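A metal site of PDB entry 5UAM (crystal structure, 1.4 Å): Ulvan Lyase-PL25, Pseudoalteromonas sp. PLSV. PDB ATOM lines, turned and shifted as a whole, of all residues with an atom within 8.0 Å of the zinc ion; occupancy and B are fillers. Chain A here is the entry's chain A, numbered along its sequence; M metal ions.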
ATOM      1  N   ASN A 132      -8.415  -2.423   2.241  1.00  0.00           N
ATOM      2  CA  ASN A 132      -8.372  -3.719   2.919  1.00  0.00           C
ATOM      3  C   ASN A 132      -9.098  -4.750   2.053  1.00  0.00           C
ATOM      4  O   ASN A 132      -9.542  -4.471   0.935  1.00  0.00           O
ATOM      5  CB  ASN A 132      -8.905  -3.593   4.352  1.00  0.00           C
ATOM      6  CG  ASN A 132     -10.393  -3.256   4.429  1.00  0.00           C
ATOM      7  OD1 ASN A 132     -10.974  -2.725   3.506  1.00  0.00           O
ATOM      8  ND2 ASN A 132     -11.009  -3.583   5.560  1.00  0.00           N
ATOM      9  N   ARG A 180     -15.348  -0.138  -5.535  1.00  0.00           N
ATOM     10  CA  ARG A 180     -14.559   0.033  -4.316  1.00  0.00           C
ATOM     11  C   ARG A 180     -13.343  -0.893  -4.367  1.00  0.00           C
ATOM     12  O   ARG A 180     -13.490  -2.087  -4.601  1.00  0.00           O
ATOM     13  CB  ARG A 180     -15.421  -0.298  -3.108  1.00  0.00           C
ATOM     14  CG  ARG A 180     -14.743  -0.068  -1.757  1.00  0.00           C
ATOM     15  CD  ARG A 180     -15.612  -0.381  -0.561  1.00  0.00           C
ATOM     16  NE  ARG A 180     -15.892  -1.819  -0.479  1.00  0.00           N
ATOM     17  CZ  ARG A 180     -16.866  -2.335   0.272  1.00  0.00           C
ATOM     18  NH1 ARG A 180     -17.646  -1.544   1.013  1.00  0.00           N
ATOM     19  NH2 ARG A 180     -17.060  -3.643   0.248  1.00  0.00           N
ATOM     20  N   ALA A 183     -12.421  -3.869   0.614  1.00  0.00           N
ATOM     21  CA  ALA A 183     -13.536  -3.874   1.552  1.00  0.00           C
ATOM     22  C   ALA A 183     -13.768  -2.458   2.100  1.00  0.00           C
ATOM     23  O   ALA A 183     -13.476  -1.482   1.409  1.00  0.00           O
ATOM     24  CB  ALA A 183     -13.292  -4.919   2.628  1.00  0.00           C
ATOM     25  N   HIS A 184     -14.331  -2.296   3.310  1.00  0.00           N
ATOM     26  CA  HIS A 184     -14.777  -0.960   3.741  1.00  0.00           C
ATOM     27  C   HIS A 184     -13.681   0.083   3.690  1.00  0.00           C
ATOM     28  O   HIS A 184     -13.947   1.247   3.344  1.00  0.00           O
ATOM     29  CB  HIS A 184     -15.256  -0.992   5.173  1.00  0.00           C
ATOM     30  CG  HIS A 184     -16.599  -1.601   5.315  1.00  0.00           C
ATOM     31  ND1 HIS A 184     -17.403  -1.370   6.405  1.00  0.00           N
ATOM     32  CD2 HIS A 184     -17.269  -2.453   4.514  1.00  0.00           C
ATOM     33  CE1 HIS A 184     -18.523  -2.060   6.262  1.00  0.00           C
ATOM     34  NE2 HIS A 184     -18.471  -2.719   5.123  1.00  0.00           N
ATOM     35  N   ARG A 185     -12.487  -0.265   4.133  1.00  0.00           N
ATOM     36  CA  ARG A 185     -11.470   0.735   4.399  1.00  0.00           C
ATOM     37  C   ARG A 185     -10.611   0.834   3.144  1.00  0.00           C
ATOM     38  O   ARG A 185      -9.419   0.506   3.124  1.00  0.00           O
ATOM     39  CB  ARG A 185     -10.716   0.397   5.670  1.00  0.00           C
ATOM     40  CG  ARG A 185     -11.658   0.478   6.873  1.00  0.00           C
ATOM     41  CD  ARG A 185     -10.984   0.234   8.203  1.00  0.00           C
ATOM     42  NE  ARG A 185     -11.858   0.662   9.291  1.00  0.00           N
ATOM     43  CZ  ARG A 185     -11.481   0.755  10.557  1.00  0.00           C
ATOM     44  NH1 ARG A 185     -10.232   0.459  10.916  1.00  0.00           N
ATOM     45  NH2 ARG A 185     -12.349   1.165  11.457  1.00  0.00           N
ATOM     46  N   VAL A 218     -12.769   5.368  10.428  1.00  0.00           N
ATOM     47  CA  VAL A 218     -12.131   5.578   9.131  1.00  0.00           C
ATOM     48  C   VAL A 218     -13.185   6.112   8.169  1.00  0.00           C
ATOM     49  O   VAL A 218     -14.338   5.651   8.190  1.00  0.00           O
ATOM     50  CB  VAL A 218     -11.522   4.246   8.612  1.00  0.00           C
ATOM     51  CG1 VAL A 218     -11.027   4.380   7.175  1.00  0.00           C
ATOM     52  CG2 VAL A 218     -10.399   3.807   9.526  1.00  0.00           C
ATOM     53  N   ASP A 219     -12.806   7.087   7.351  1.00  0.00           N
ATOM     54  CA  ASP A 219     -13.681   7.547   6.288  1.00  0.00           C
ATOM     55  C   ASP A 219     -13.885   6.422   5.272  1.00  0.00           C
ATOM     56  O   ASP A 219     -12.910   5.839   4.785  1.00  0.00           O
ATOM     57  CB  ASP A 219     -13.075   8.742   5.534  1.00  0.00           C
ATOM     58  CG  ASP A 219     -12.970  10.011   6.370  1.00  0.00           C
ATOM     59  OD1 ASP A 219     -13.695  10.211   7.369  1.00  0.00           O
ATOM     60  OD2 ASP A 219     -12.123  10.845   5.973  1.00  0.00           O
ATOM     61  N   SER A 220     -15.136   6.156   4.938  1.00  0.00           N
ATOM     62  CA  SER A 220     -15.521   5.093   4.015  1.00  0.00           C
ATOM     63  C   SER A 220     -16.715   5.598   3.228  1.00  0.00           C
ATOM     64  O   SER A 220     -17.403   6.537   3.655  1.00  0.00           O
ATOM     65  CB  SER A 220     -15.849   3.833   4.819  1.00  0.00           C
ATOM     66  OG  SER A 220     -16.133   2.710   4.022  1.00  0.00           O
ATOM     67  N   TRP A 221     -16.962   4.985   2.063  1.00  0.00           N
ATOM     68  CA  TRP A 221     -17.919   5.544   1.116  1.00  0.00           C
ATOM     69  C   TRP A 221     -18.709   4.460   0.393  1.00  0.00           C
ATOM     70  O   TRP A 221     -18.268   3.317   0.285  1.00  0.00           O
ATOM     71  CB  TRP A 221     -17.203   6.347   0.036  1.00  0.00           C
ATOM     72  CG  TRP A 221     -16.351   7.459   0.566  1.00  0.00           C
ATOM     73  CD1 TRP A 221     -14.982   7.430   0.791  1.00  0.00           C
ATOM     74  CD2 TRP A 221     -16.794   8.773   0.910  1.00  0.00           C
ATOM     75  NE1 TRP A 221     -14.571   8.659   1.253  1.00  0.00           N
ATOM     76  CE2 TRP A 221     -15.658   9.497   1.346  1.00  0.00           C
ATOM     77  CE3 TRP A 221     -18.038   9.409   0.894  1.00  0.00           C
ATOM     78  CZ2 TRP A 221     -15.741  10.823   1.747  1.00  0.00           C
ATOM     79  CZ3 TRP A 221     -18.125  10.726   1.310  1.00  0.00           C
ATOM     80  CH2 TRP A 221     -16.982  11.417   1.729  1.00  0.00           C
ATOM     81  N   TYR A 222     -19.852   4.875  -0.169  1.00  0.00           N
ATOM     82  CA  TYR A 222     -20.586   4.062  -1.138  1.00  0.00           C
ATOM     83  C   TYR A 222     -21.034   4.971  -2.270  1.00  0.00           C
ATOM     84  O   TYR A 222     -21.660   6.015  -2.026  1.00  0.00           O
ATOM     85  CB  TYR A 222     -21.808   3.403  -0.501  1.00  0.00           C
ATOM     86  CG  TYR A 222     -21.451   2.340   0.508  1.00  0.00           C
ATOM     87  CD1 TYR A 222     -21.243   2.675   1.845  1.00  0.00           C
ATOM     88  CD2 TYR A 222     -21.293   1.008   0.139  1.00  0.00           C
ATOM     89  CE1 TYR A 222     -20.879   1.717   2.779  1.00  0.00           C
ATOM     90  CE2 TYR A 222     -20.945   0.048   1.054  1.00  0.00           C
ATOM     91  CZ  TYR A 222     -20.758   0.400   2.395  1.00  0.00           C
ATOM     92  OH  TYR A 222     -20.401  -0.553   3.323  1.00  0.00           O
ATOM     93  N   HIS A 240     -19.887   6.445   4.940  1.00  0.00           N
ATOM     94  CA  HIS A 240     -19.917   5.411   5.970  1.00  0.00           C
ATOM     95  C   HIS A 240     -18.931   5.801   7.085  1.00  0.00           C
ATOM     96  O   HIS A 240     -17.731   5.965   6.828  1.00  0.00           O
ATOM     97  CB  HIS A 240     -19.564   4.060   5.344  1.00  0.00           C
ATOM     98  CG  HIS A 240     -19.313   2.964   6.324  1.00  0.00           C
ATOM     99  ND1 HIS A 240     -20.153   2.682   7.381  1.00  0.00           N
ATOM    100  CD2 HIS A 240     -18.312   2.052   6.397  1.00  0.00           C
ATOM    101  CE1 HIS A 240     -19.683   1.660   8.069  1.00  0.00           C
ATOM    102  NE2 HIS A 240     -18.566   1.251   7.483  1.00  0.00           N
ATOM    103  N   VAL A 241     -19.458   5.973   8.297  1.00  0.00           N
ATOM    104  CA  VAL A 241     -18.638   6.117   9.495  1.00  0.00           C
ATOM    105  C   VAL A 241     -18.171   4.702   9.843  1.00  0.00           C
ATOM    106  O   VAL A 241     -18.938   3.918  10.410  1.00  0.00           O
ATOM    107  CB  VAL A 241     -19.432   6.717  10.665  1.00  0.00           C
ATOM    108  CG1 VAL A 241     -18.467   7.062  11.816  1.00  0.00           C
ATOM    109  CG2 VAL A 241     -20.292   7.902  10.240  1.00  0.00           C
ATOM    110  N   CYS A 242     -16.928   4.378   9.523  1.00  0.00           N
ATOM    111  CA  CYS A 242     -16.439   3.022   9.678  1.00  0.00           C
ATOM    112  C   CYS A 242     -15.701   2.933  11.013  1.00  0.00           C
ATOM    113  O   CYS A 242     -14.496   3.181  11.118  1.00  0.00           O
ATOM    114  CB  CYS A 242     -15.585   2.615   8.480  1.00  0.00           C
ATOM    115  SG  CYS A 242     -15.150   0.858   8.510  1.00  0.00           S
ATOM    116  N   TRP A 243     -16.445   2.560  12.046  1.00  0.00           N
ATOM    117  CA  TRP A 243     -15.945   2.613  13.414  1.00  0.00           C
ATOM    118  C   TRP A 243     -14.961   1.485  13.702  1.00  0.00           C
ATOM    119  O   TRP A 243     -15.143   0.355  13.240  1.00  0.00           O
ATOM    120  CB  TRP A 243     -17.115   2.462  14.396  1.00  0.00           C
ATOM    121  CG  TRP A 243     -18.010   3.660  14.499  1.00  0.00           C
ATOM    122  CD1 TRP A 243     -19.248   3.828  13.911  1.00  0.00           C
ATOM    123  CD2 TRP A 243     -17.759   4.844  15.246  1.00  0.00           C
ATOM    124  NE1 TRP A 243     -19.766   5.049  14.261  1.00  0.00           N
ATOM    125  CE2 TRP A 243     -18.871   5.698  15.079  1.00  0.00           C
ATOM    126  CE3 TRP A 243     -16.700   5.282  16.038  1.00  0.00           C
ATOM    127  CZ2 TRP A 243     -18.947   6.954  15.683  1.00  0.00           C
ATOM    128  CZ3 TRP A 243     -16.782   6.531  16.642  1.00  0.00           C
ATOM    129  CH2 TRP A 243     -17.889   7.352  16.444  1.00  0.00           C
ATOM    130  N   ASP A 244     -13.929   1.803  14.477  1.00  0.00           N
ATOM    131  CA  ASP A 244     -13.059   0.771  15.029  1.00  0.00           C
ATOM    132  C   ASP A 244     -13.866  -0.094  15.991  1.00  0.00           C
ATOM    133  O   ASP A 244     -14.836   0.365  16.607  1.00  0.00           O
ATOM    134  CB  ASP A 244     -11.910   1.408  15.831  1.00  0.00           C
ATOM    135  CG  ASP A 244     -10.898   2.129  14.969  1.00  0.00           C
ATOM    136  OD1 ASP A 244     -10.968   2.036  13.724  1.00  0.00           O
ATOM    137  OD2 ASP A 244     -10.019   2.787  15.560  1.00  0.00           O
ATOM    138  N   HIS A 254     -18.418  -1.468  15.404  1.00  0.00           N
ATOM    139  CA  HIS A 254     -18.597  -1.306  13.978  1.00  0.00           C
ATOM    140  C   HIS A 254     -20.014  -1.676  13.555  1.00  0.00           C
ATOM    141  O   HIS A 254     -20.491  -2.777  13.830  1.00  0.00           O
ATOM    142  CB  HIS A 254     -17.592  -2.151  13.203  1.00  0.00           C
ATOM    143  CG  HIS A 254     -17.735  -1.970  11.737  1.00  0.00           C
ATOM    144  ND1 HIS A 254     -18.568  -2.742  10.956  1.00  0.00           N
ATOM    145  CD2 HIS A 254     -17.230  -1.020  10.915  1.00  0.00           C
ATOM    146  CE1 HIS A 254     -18.540  -2.298   9.714  1.00  0.00           C
ATOM    147  NE2 HIS A 254     -17.736  -1.252   9.661  1.00  0.00           N
ATOM    148  N   THR A 255     -20.680  -0.740  12.877  1.00  0.00           N
ATOM    149  CA  THR A 255     -22.035  -0.935  12.361  1.00  0.00           C
ATOM    150  C   THR A 255     -22.065  -0.577  10.880  1.00  0.00           C
ATOM    151  O   THR A 255     -21.032  -0.291  10.267  1.00  0.00           O
ATOM    152  CB  THR A 255     -23.012  -0.013  13.099  1.00  0.00           C
ATOM    153  OG1 THR A 255     -22.657   1.338  12.802  1.00  0.00           O
ATOM    154  CG2 THR A 255     -23.011  -0.268  14.624  1.00  0.00           C
ATOM    155  N   THR A 256     -23.259  -0.546  10.286  1.00  0.00           N
ATOM    156  CA  THR A 256     -23.418  -0.077   8.914  1.00  0.00           C
ATOM    157  C   THR A 256     -23.736   1.417   8.834  1.00  0.00           C
ATOM    158  O   THR A 256     -24.249   1.873   7.813  1.00  0.00           O
ATOM    159  CB  THR A 256     -24.513  -0.854   8.177  1.00  0.00           C
ATOM    160  OG1 THR A 256     -25.775  -0.634   8.817  1.00  0.00           O
ATOM    161  CG2 THR A 256     -24.209  -2.330   8.152  1.00  0.00           C
ATOM    162  N   GLU A 257     -23.444   2.179   9.885  1.00  0.00           N
ATOM    163  CA  GLU A 257     -23.794   3.592   9.942  1.00  0.00           C
ATOM    164  C   GLU A 257     -23.319   4.346   8.715  1.00  0.00           C
ATOM    165  O   GLU A 257     -22.120   4.392   8.418  1.00  0.00           O
ATOM    166  CB  GLU A 257     -23.182   4.214  11.206  1.00  0.00           C
ATOM    167  CG  GLU A 257     -23.626   5.661  11.406  1.00  0.00           C
ATOM    168  CD  GLU A 257     -23.120   6.293  12.693  1.00  0.00           C
ATOM    169  OE1 GLU A 257     -22.631   5.565  13.591  1.00  0.00           O
ATOM    170  OE2 GLU A 257     -23.260   7.530  12.819  1.00  0.00           O
ATOM    171  N   ARG A 258     -24.266   4.966   8.006  1.00  0.00           N
ATOM    172  CA  ARG A 258     -23.990   5.808   6.861  1.00  0.00           C
ATOM    173  C   ARG A 258     -24.887   7.034   6.972  1.00  0.00           C
ATOM    174  O   ARG A 258     -25.974   6.942   7.531  1.00  0.00           O
ATOM    175  CB  ARG A 258     -24.284   5.081   5.540  1.00  0.00           C
ATOM    176  CG  ARG A 258     -23.415   3.844   5.317  1.00  0.00           C
ATOM    177  CD  ARG A 258     -24.089   2.773   4.463  1.00  0.00           C
ATOM    178  NE  ARG A 258     -24.354   3.212   3.098  1.00  0.00           N
ATOM    179  CZ  ARG A 258     -24.502   2.400   2.053  1.00  0.00           C
ATOM    180  NH1 ARG A 258     -24.421   1.087   2.196  1.00  0.00           N
ATOM    181  NH2 ARG A 258     -24.703   2.927   0.854  1.00  0.00           N
HETATM  182 ZN    ZN M   1     -17.155  -0.123   8.035  1.00  0.00          ZN
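The zinc ion is bound by a ring nitrogen (NE2) of His 240 (2.0 Å), a ring nitrogen (NE2) of His 254 (2.1 Å), a ring nitrogen (ND1) of His 184 (2.1 Å) and the side-chain sulfur (SG) of Cys 242 (2.3 Å).
A ring nitrogen (ND1) of His 240 lies within hydrogen-bond range of the backbone carbonyl oxygen of Glu 257, 2.8 Å away.
The backbone carbonyl oxygen of Cys 242 sits at hydrogen-bond distance from the guanidinium group of Arg 185 (3.0 Å).
The backbone carbonyl oxygen (O) of Cys 242 lies within hydrogen-bond range of the backbone NH (N) of Val 218.
The backbone carbonyl oxygen of Ser 220 lies within hydrogen-bond range of the backbone NH of His 240.
The backbone NH (N) of His 184 lies within hydrogen-bond range of the side-chain amide oxygen (OD1) of Asn 132 (3.4 Å).
O of His 184 is in hydrogen-bond range of OG of Ser 220.
NE2 of His 184 sits at hydrogen-bond distance from OH of Tyr 222 (3.4 Å).
Of the 20 residues printed, 4 come within 4 Å of the zinc ion.
The nearest printed residue that does not touch the zinc ion is Thr 255 (4.5 Å).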
